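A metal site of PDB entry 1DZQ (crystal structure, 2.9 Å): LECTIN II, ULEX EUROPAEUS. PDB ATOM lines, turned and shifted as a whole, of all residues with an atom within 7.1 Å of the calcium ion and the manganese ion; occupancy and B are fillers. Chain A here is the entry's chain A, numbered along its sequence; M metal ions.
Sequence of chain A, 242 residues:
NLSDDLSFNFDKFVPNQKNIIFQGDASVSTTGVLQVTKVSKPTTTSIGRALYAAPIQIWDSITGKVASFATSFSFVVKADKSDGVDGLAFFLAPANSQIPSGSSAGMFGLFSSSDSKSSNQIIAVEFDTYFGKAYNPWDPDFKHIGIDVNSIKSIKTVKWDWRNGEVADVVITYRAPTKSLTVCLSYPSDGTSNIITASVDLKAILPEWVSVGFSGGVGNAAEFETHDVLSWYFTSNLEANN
The calcium ion is bound by the side-chain carboxylate (OD1) of Asp 128 (2.3 Å), the side-chain amide oxygen (OD1) of Asn 136 (2.3 Å), the backbone carbonyl oxygen (O) of Tyr 130 (2.5 Å), the side-chain carboxylate (OD2) of Asp 139 (2.5 Å) and the side-chain carboxylate (OD2) of Asp 128 (2.7 Å).
The side-chain carboxylate (OD1) of Asp 139 is bound to the manganese ion (2.0 Å).
The manganese ion is bound by the side-chain carboxylate (OD2) of Asp 128, at 2.1 Å.
OE2 of Glu 126 binds the manganese ion (2.1 Å).
NE2 of His 144 binds the manganese ion (2.2 Å).
Four residues have an atom within 4 Å of the calcium ion: Asp 128, Tyr 130, Asn 136 and Asp 139.
Along chain A the residues within 4 Å of the calcium ion span positions 128 to 139.
NE1 of Trp 138 lies close to OD2 of Asp 139 (3.4 Å).
The backbone carbonyl oxygen (O) of Gly 146 sits at hydrogen-bond distance from the backbone NH (N) of Glu 126, 2.9 Å away.
The side-chain carboxylate of Asp 148 lies close to the side-chain carboxylate of Glu 126 (2.6 Å).
OG of Ser 154 is in hydrogen-bond range of OD1 of Asp 148, 2.7 Å away.
O of Phe 142 is in hydrogen-bond range of ND1 of His 144 (2.8 Å).
Ser 154 touches the manganese ion.
Within 4 Å of the manganese ion: Glu 126, Asp 128, Asp 139, His 144 and Ser 154.
The nearest printed residue that does not touch the manganese ion is Ile 152 (4.4 Å).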
ATOM      1  N   ASP A  86     -15.911 -27.970 -35.751  1.00  0.00           N
ATOM      2  CA  ASP A  86     -15.070 -28.109 -34.573  1.00  0.00           C
ATOM      3  C   ASP A  86     -13.725 -27.408 -34.714  1.00  0.00           C
ATOM      4  O   ASP A  86     -13.042 -27.136 -33.712  1.00  0.00           O
ATOM      5  CB  ASP A  86     -14.799 -29.581 -34.328  1.00  0.00           C
ATOM      6  CG  ASP A  86     -15.447 -30.069 -33.081  1.00  0.00           C
ATOM      7  OD1 ASP A  86     -16.643 -30.415 -33.162  1.00  0.00           O
ATOM      8  OD2 ASP A  86     -14.777 -30.087 -32.031  1.00  0.00           O
ATOM      9  N   GLY A  87     -13.302 -27.197 -35.960  1.00  0.00           N
ATOM     10  CA  GLY A  87     -12.019 -26.567 -36.205  1.00  0.00           C
ATOM     11  C   GLY A  87     -11.290 -27.157 -37.403  1.00  0.00           C
ATOM     12  O   GLY A  87     -11.749 -28.116 -38.022  1.00  0.00           O
ATOM     13  N   ALA A 105     -14.393 -35.584 -34.359  1.00  0.00           N
ATOM     14  CA  ALA A 105     -14.211 -34.265 -34.954  1.00  0.00           C
ATOM     15  C   ALA A 105     -13.362 -33.383 -34.036  1.00  0.00           C
ATOM     16  O   ALA A 105     -12.524 -32.604 -34.509  1.00  0.00           O
ATOM     17  CB  ALA A 105     -15.541 -33.615 -35.213  1.00  0.00           C
ATOM     18  N   GLY A 106     -13.574 -33.521 -32.732  1.00  0.00           N
ATOM     19  CA  GLY A 106     -12.818 -32.732 -31.766  1.00  0.00           C
ATOM     20  C   GLY A 106     -11.328 -33.029 -31.773  1.00  0.00           C
ATOM     21  O   GLY A 106     -10.538 -32.282 -31.198  1.00  0.00           O
ATOM     22  N   MET A 107     -10.959 -34.147 -32.399  1.00  0.00           N
ATOM     23  CA  MET A 107      -9.554 -34.543 -32.514  1.00  0.00           C
ATOM     24  C   MET A 107      -9.059 -34.375 -33.951  1.00  0.00           C
ATOM     25  O   MET A 107      -7.943 -34.754 -34.288  1.00  0.00           O
ATOM     26  CB  MET A 107      -9.361 -35.953 -31.983  1.00  0.00           C
ATOM     27  CG  MET A 107      -9.778 -36.047 -30.536  1.00  0.00           C
ATOM     28  SD  MET A 107      -9.508 -37.608 -29.735  1.00  0.00           S
ATOM     29  CE  MET A 107     -10.863 -38.619 -30.466  1.00  0.00           C
ATOM     30  N   PHE A 108      -9.915 -33.772 -34.777  1.00  0.00           N
ATOM     31  CA  PHE A 108      -9.634 -33.464 -36.179  1.00  0.00           C
ATOM     32  C   PHE A 108      -9.172 -34.630 -37.035  1.00  0.00           C
ATOM     33  O   PHE A 108      -8.480 -34.430 -38.044  1.00  0.00           O
ATOM     34  CB  PHE A 108      -8.615 -32.323 -36.252  1.00  0.00           C
ATOM     35  CG  PHE A 108      -8.946 -31.159 -35.366  1.00  0.00           C
ATOM     36  CD1 PHE A 108     -10.087 -30.390 -35.578  1.00  0.00           C
ATOM     37  CD2 PHE A 108      -8.109 -30.820 -34.298  1.00  0.00           C
ATOM     38  CE1 PHE A 108     -10.396 -29.318 -34.742  1.00  0.00           C
ATOM     39  CE2 PHE A 108      -8.409 -29.751 -33.458  1.00  0.00           C
ATOM     40  CZ  PHE A 108      -9.553 -29.000 -33.680  1.00  0.00           C
ATOM     41  N   GLU A 126      -3.477 -26.290 -34.851  1.00  0.00           N
ATOM     42  CA  GLU A 126      -4.916 -26.295 -34.898  1.00  0.00           C
ATOM     43  C   GLU A 126      -5.542 -24.916 -34.774  1.00  0.00           C
ATOM     44  O   GLU A 126      -4.977 -24.019 -34.155  1.00  0.00           O
ATOM     45  CB  GLU A 126      -5.471 -27.204 -33.793  1.00  0.00           C
ATOM     46  CG  GLU A 126      -5.007 -26.830 -32.394  1.00  0.00           C
ATOM     47  CD  GLU A 126      -5.860 -27.434 -31.298  1.00  0.00           C
ATOM     48  OE1 GLU A 126      -5.877 -28.673 -31.140  1.00  0.00           O
ATOM     49  OE2 GLU A 126      -6.541 -26.658 -30.592  1.00  0.00           O
ATOM     50  N   PHE A 127      -6.701 -24.766 -35.404  1.00  0.00           N
ATOM     51  CA  PHE A 127      -7.494 -23.540 -35.353  1.00  0.00           C
ATOM     52  C   PHE A 127      -8.815 -24.079 -34.805  1.00  0.00           C
ATOM     53  O   PHE A 127      -9.728 -24.428 -35.563  1.00  0.00           O
ATOM     54  CB  PHE A 127      -7.629 -22.953 -36.746  1.00  0.00           C
ATOM     55  CG  PHE A 127      -6.324 -22.598 -37.374  1.00  0.00           C
ATOM     56  CD1 PHE A 127      -5.715 -21.369 -37.119  1.00  0.00           C
ATOM     57  CD2 PHE A 127      -5.663 -23.511 -38.181  1.00  0.00           C
ATOM     58  CE1 PHE A 127      -4.469 -21.058 -37.652  1.00  0.00           C
ATOM     59  CE2 PHE A 127      -4.405 -23.209 -38.722  1.00  0.00           C
ATOM     60  CZ  PHE A 127      -3.815 -21.983 -38.456  1.00  0.00           C
ATOM     61  N   ASP A 128      -8.835 -24.233 -33.483  1.00  0.00           N
ATOM     62  CA  ASP A 128      -9.941 -24.782 -32.685  1.00  0.00           C
ATOM     63  C   ASP A 128     -11.090 -23.813 -32.445  1.00  0.00           C
ATOM     64  O   ASP A 128     -10.928 -22.809 -31.763  1.00  0.00           O
ATOM     65  CB  ASP A 128      -9.354 -25.217 -31.338  1.00  0.00           C
ATOM     66  CG  ASP A 128     -10.009 -26.440 -30.763  1.00  0.00           C
ATOM     67  OD1 ASP A 128     -11.184 -26.703 -31.084  1.00  0.00           O
ATOM     68  OD2 ASP A 128      -9.325 -27.144 -29.978  1.00  0.00           O
ATOM     69  N   THR A 129     -12.272 -24.147 -32.947  1.00  0.00           N
ATOM     70  CA  THR A 129     -13.447 -23.288 -32.774  1.00  0.00           C
ATOM     71  C   THR A 129     -14.363 -23.711 -31.633  1.00  0.00           C
ATOM     72  O   THR A 129     -15.184 -22.908 -31.166  1.00  0.00           O
ATOM     73  CB  THR A 129     -14.290 -23.221 -34.051  1.00  0.00           C
ATOM     74  OG1 THR A 129     -14.607 -24.551 -34.476  1.00  0.00           O
ATOM     75  CG2 THR A 129     -13.552 -22.502 -35.156  1.00  0.00           C
ATOM     76  N   TYR A 130     -14.263 -24.966 -31.209  1.00  0.00           N
ATOM     77  CA  TYR A 130     -15.084 -25.481 -30.117  1.00  0.00           C
ATOM     78  C   TYR A 130     -14.210 -25.763 -28.897  1.00  0.00           C
ATOM     79  O   TYR A 130     -13.196 -26.463 -29.002  1.00  0.00           O
ATOM     80  CB  TYR A 130     -15.819 -26.750 -30.536  1.00  0.00           C
ATOM     81  CG  TYR A 130     -16.594 -27.393 -29.412  1.00  0.00           C
ATOM     82  CD1 TYR A 130     -17.830 -26.880 -29.014  1.00  0.00           C
ATOM     83  CD2 TYR A 130     -16.089 -28.499 -28.726  1.00  0.00           C
ATOM     84  CE1 TYR A 130     -18.543 -27.455 -27.946  1.00  0.00           C
ATOM     85  CE2 TYR A 130     -16.788 -29.075 -27.662  1.00  0.00           C
ATOM     86  CZ  TYR A 130     -18.006 -28.543 -27.281  1.00  0.00           C
ATOM     87  OH  TYR A 130     -18.709 -29.120 -26.233  1.00  0.00           O
ATOM     88  N   PHE A 131     -14.652 -25.289 -27.736  1.00  0.00           N
ATOM     89  CA  PHE A 131     -13.897 -25.476 -26.510  1.00  0.00           C
ATOM     90  C   PHE A 131     -14.747 -25.889 -25.302  1.00  0.00           C
ATOM     91  O   PHE A 131     -14.312 -25.748 -24.159  1.00  0.00           O
ATOM     92  CB  PHE A 131     -13.119 -24.204 -26.190  1.00  0.00           C
ATOM     93  CG  PHE A 131     -13.982 -22.978 -26.099  1.00  0.00           C
ATOM     94  CD1 PHE A 131     -14.380 -22.299 -27.250  1.00  0.00           C
ATOM     95  CD2 PHE A 131     -14.432 -22.518 -24.869  1.00  0.00           C
ATOM     96  CE1 PHE A 131     -15.200 -21.186 -27.176  1.00  0.00           C
ATOM     97  CE2 PHE A 131     -15.256 -21.399 -24.782  1.00  0.00           C
ATOM     98  CZ  PHE A 131     -15.646 -20.733 -25.934  1.00  0.00           C
ATOM     99  N   GLY A 132     -15.958 -26.391 -25.555  1.00  0.00           N
ATOM    100  CA  GLY A 132     -16.836 -26.799 -24.472  1.00  0.00           C
ATOM    101  C   GLY A 132     -16.184 -27.792 -23.533  1.00  0.00           C
ATOM    102  O   GLY A 132     -15.704 -28.839 -23.964  1.00  0.00           O
ATOM    103  N   ASN A 136     -14.672 -31.212 -24.698  1.00  0.00           N
ATOM    104  CA  ASN A 136     -13.256 -30.945 -24.951  1.00  0.00           C
ATOM    105  C   ASN A 136     -12.599 -30.389 -23.684  1.00  0.00           C
ATOM    106  O   ASN A 136     -12.145 -29.237 -23.660  1.00  0.00           O
ATOM    107  CB  ASN A 136     -13.095 -29.913 -26.085  1.00  0.00           C
ATOM    108  CG  ASN A 136     -13.336 -30.504 -27.466  1.00  0.00           C
ATOM    109  OD1 ASN A 136     -12.984 -29.887 -28.467  1.00  0.00           O
ATOM    110  ND2 ASN A 136     -13.938 -31.679 -27.532  1.00  0.00           N
ATOM    111  N   TRP A 138      -9.735 -30.614 -22.459  1.00  0.00           N
ATOM    112  CA  TRP A 138      -8.335 -30.212 -22.638  1.00  0.00           C
ATOM    113  C   TRP A 138      -8.167 -28.775 -23.152  1.00  0.00           C
ATOM    114  O   TRP A 138      -7.112 -28.170 -22.956  1.00  0.00           O
ATOM    115  CB  TRP A 138      -7.645 -31.194 -23.599  1.00  0.00           C
ATOM    116  CG  TRP A 138      -8.400 -31.343 -24.906  1.00  0.00           C
ATOM    117  CD1 TRP A 138      -8.434 -30.468 -25.951  1.00  0.00           C
ATOM    118  CD2 TRP A 138      -9.274 -32.416 -25.264  1.00  0.00           C
ATOM    119  NE1 TRP A 138      -9.283 -30.913 -26.928  1.00  0.00           N
ATOM    120  CE2 TRP A 138      -9.810 -32.116 -26.527  1.00  0.00           C
ATOM    121  CE3 TRP A 138      -9.662 -33.607 -24.634  1.00  0.00           C
ATOM    122  CZ2 TRP A 138     -10.723 -32.960 -27.184  1.00  0.00           C
ATOM    123  CZ3 TRP A 138     -10.557 -34.450 -25.278  1.00  0.00           C
ATOM    124  CH2 TRP A 138     -11.077 -34.117 -26.541  1.00  0.00           C
ATOM    125  N   ASP A 139      -9.183 -28.271 -23.837  1.00  0.00           N
ATOM    126  CA  ASP A 139      -9.171 -26.924 -24.414  1.00  0.00           C
ATOM    127  C   ASP A 139      -9.280 -25.780 -23.410  1.00  0.00           C
ATOM    128  O   ASP A 139      -9.737 -25.974 -22.289  1.00  0.00           O
ATOM    129  CB  ASP A 139     -10.314 -26.787 -25.422  1.00  0.00           C
ATOM    130  CG  ASP A 139      -9.948 -27.370 -26.782  1.00  0.00           C
ATOM    131  OD1 ASP A 139      -8.759 -27.303 -27.213  1.00  0.00           O
ATOM    132  OD2 ASP A 139     -10.842 -27.948 -27.362  1.00  0.00           O
ATOM    133  N   PRO A 140      -8.695 -24.602 -23.739  1.00  0.00           N
ATOM    134  CA  PRO A 140      -8.787 -23.395 -22.894  1.00  0.00           C
ATOM    135  C   PRO A 140     -10.181 -22.799 -23.080  1.00  0.00           C
ATOM    136  O   PRO A 140     -10.953 -23.310 -23.896  1.00  0.00           O
ATOM    137  CB  PRO A 140      -7.688 -22.495 -23.450  1.00  0.00           C
ATOM    138  CG  PRO A 140      -7.629 -22.889 -24.877  1.00  0.00           C
ATOM    139  CD  PRO A 140      -7.685 -24.381 -24.793  1.00  0.00           C
ATOM    140  N   PHE A 142     -11.622 -20.393 -24.783  1.00  0.00           N
ATOM    141  CA  PHE A 142     -11.804 -19.515 -25.937  1.00  0.00           C
ATOM    142  C   PHE A 142     -11.365 -20.189 -27.216  1.00  0.00           C
ATOM    143  O   PHE A 142     -10.656 -21.205 -27.185  1.00  0.00           O
ATOM    144  CB  PHE A 142     -11.017 -18.210 -25.741  1.00  0.00           C
ATOM    145  CG  PHE A 142      -9.605 -18.420 -25.240  1.00  0.00           C
ATOM    146  CD1 PHE A 142      -8.588 -18.845 -26.109  1.00  0.00           C
ATOM    147  CD2 PHE A 142      -9.291 -18.222 -23.897  1.00  0.00           C
ATOM    148  CE1 PHE A 142      -7.294 -19.061 -25.645  1.00  0.00           C
ATOM    149  CE2 PHE A 142      -7.995 -18.429 -23.429  1.00  0.00           C
ATOM    150  CZ  PHE A 142      -7.001 -18.859 -24.304  1.00  0.00           C
ATOM    151  N   HIS A 144      -9.107 -20.900 -30.076  1.00  0.00           N
ATOM    152  CA  HIS A 144      -7.663 -20.739 -30.063  1.00  0.00           C
ATOM    153  C   HIS A 144      -6.887 -21.312 -31.244  1.00  0.00           C
ATOM    154  O   HIS A 144      -7.439 -21.959 -32.127  1.00  0.00           O
ATOM    155  CB  HIS A 144      -7.129 -21.403 -28.789  1.00  0.00           C
ATOM    156  CG  HIS A 144      -7.617 -22.813 -28.609  1.00  0.00           C
ATOM    157  ND1 HIS A 144      -8.895 -23.114 -28.189  1.00  0.00           N
ATOM    158  CD2 HIS A 144      -7.015 -24.000 -28.865  1.00  0.00           C
ATOM    159  CE1 HIS A 144      -9.060 -24.422 -28.199  1.00  0.00           C
ATOM    160  NE2 HIS A 144      -7.937 -24.980 -28.609  1.00  0.00           N
ATOM    161  N   ILE A 145      -5.587 -21.019 -31.240  1.00  0.00           N
ATOM    162  CA  ILE A 145      -4.647 -21.524 -32.215  1.00  0.00           C
ATOM    163  C   ILE A 145      -3.719 -22.301 -31.305  1.00  0.00           C
ATOM    164  O   ILE A 145      -3.227 -21.761 -30.315  1.00  0.00           O
ATOM    165  CB  ILE A 145      -3.819 -20.406 -32.878  1.00  0.00           C
ATOM    166  CG1 ILE A 145      -4.713 -19.500 -33.719  1.00  0.00           C
ATOM    167  CG2 ILE A 145      -2.711 -21.024 -33.737  1.00  0.00           C
ATOM    168  CD1 ILE A 145      -3.951 -18.369 -34.387  1.00  0.00           C
ATOM    169  N   GLY A 146      -3.491 -23.578 -31.604  1.00  0.00           N
ATOM    170  CA  GLY A 146      -2.625 -24.355 -30.740  1.00  0.00           C
ATOM    171  C   GLY A 146      -1.612 -25.190 -31.473  1.00  0.00           C
ATOM    172  O   GLY A 146      -1.868 -25.653 -32.584  1.00  0.00           O
ATOM    173  N   ASP A 148       0.082 -28.528 -31.487  1.00  0.00           N
ATOM    174  CA  ASP A 148      -0.117 -29.855 -30.934  1.00  0.00           C
ATOM    175  C   ASP A 148       1.055 -30.752 -31.246  1.00  0.00           C
ATOM    176  O   ASP A 148       1.489 -30.836 -32.401  1.00  0.00           O
ATOM    177  CB  ASP A 148      -1.386 -30.501 -31.494  1.00  0.00           C
ATOM    178  CG  ASP A 148      -2.632 -29.710 -31.179  1.00  0.00           C
ATOM    179  OD1 ASP A 148      -2.569 -28.721 -30.419  1.00  0.00           O
ATOM    180  OD2 ASP A 148      -3.698 -30.068 -31.711  1.00  0.00           O
ATOM    181  N   ILE A 152      -3.851 -33.996 -28.506  1.00  0.00           N
ATOM    182  CA  ILE A 152      -4.869 -32.996 -28.816  1.00  0.00           C
ATOM    183  C   ILE A 152      -4.835 -31.855 -27.785  1.00  0.00           C
ATOM    184  O   ILE A 152      -5.475 -30.812 -27.965  1.00  0.00           O
ATOM    185  CB  ILE A 152      -6.279 -33.629 -28.904  1.00  0.00           C
ATOM    186  CG1 ILE A 152      -7.276 -32.648 -29.538  1.00  0.00           C
ATOM    187  CG2 ILE A 152      -6.747 -34.086 -27.535  1.00  0.00           C
ATOM    188  CD1 ILE A 152      -6.932 -32.257 -30.962  1.00  0.00           C
ATOM    189  N   LYS A 153      -4.118 -32.090 -26.689  1.00  0.00           N
ATOM    190  CA  LYS A 153      -3.945 -31.099 -25.633  1.00  0.00           C
ATOM    191  C   LYS A 153      -2.680 -30.338 -26.047  1.00  0.00           C
ATOM    192  O   LYS A 153      -1.554 -30.830 -25.870  1.00  0.00           O
ATOM    193  CB  LYS A 153      -3.769 -31.776 -24.276  1.00  0.00           C
ATOM    194  CG  LYS A 153      -3.515 -30.800 -23.113  1.00  0.00           C
ATOM    195  CD  LYS A 153      -3.514 -31.509 -21.756  1.00  0.00           C
ATOM    196  CE  LYS A 153      -2.956 -30.614 -20.653  1.00  0.00           C
ATOM    197  NZ  LYS A 153      -3.683 -29.314 -20.547  1.00  0.00           N
ATOM    198  N   SER A 154      -2.894 -29.186 -26.667  1.00  0.00           N
ATOM    199  CA  SER A 154      -1.844 -28.314 -27.180  1.00  0.00           C
ATOM    200  C   SER A 154      -0.806 -27.978 -26.122  1.00  0.00           C
ATOM    201  O   SER A 154      -1.140 -27.800 -24.957  1.00  0.00           O
ATOM    202  CB  SER A 154      -2.456 -27.028 -27.722  1.00  0.00           C
ATOM    203  OG  SER A 154      -3.700 -27.263 -28.386  1.00  0.00           O
ATOM    204  N   THR A 157      -1.035 -22.453 -26.567  1.00  0.00           N
ATOM    205  CA  THR A 157      -2.150 -21.888 -27.313  1.00  0.00           C
ATOM    206  C   THR A 157      -2.150 -20.366 -27.226  1.00  0.00           C
ATOM    207  O   THR A 157      -1.368 -19.775 -26.473  1.00  0.00           O
ATOM    208  CB  THR A 157      -3.522 -22.389 -26.798  1.00  0.00           C
ATOM    209  OG1 THR A 157      -3.705 -21.956 -25.448  1.00  0.00           O
ATOM    210  CG2 THR A 157      -3.595 -23.903 -26.857  1.00  0.00           C
HETATM  211 CA    CA M   1     -11.758 -28.389 -29.698  1.00  0.00          CA
HETATM  212 MN    MN M   2      -7.592 -27.115 -28.853  1.00  0.00          MN
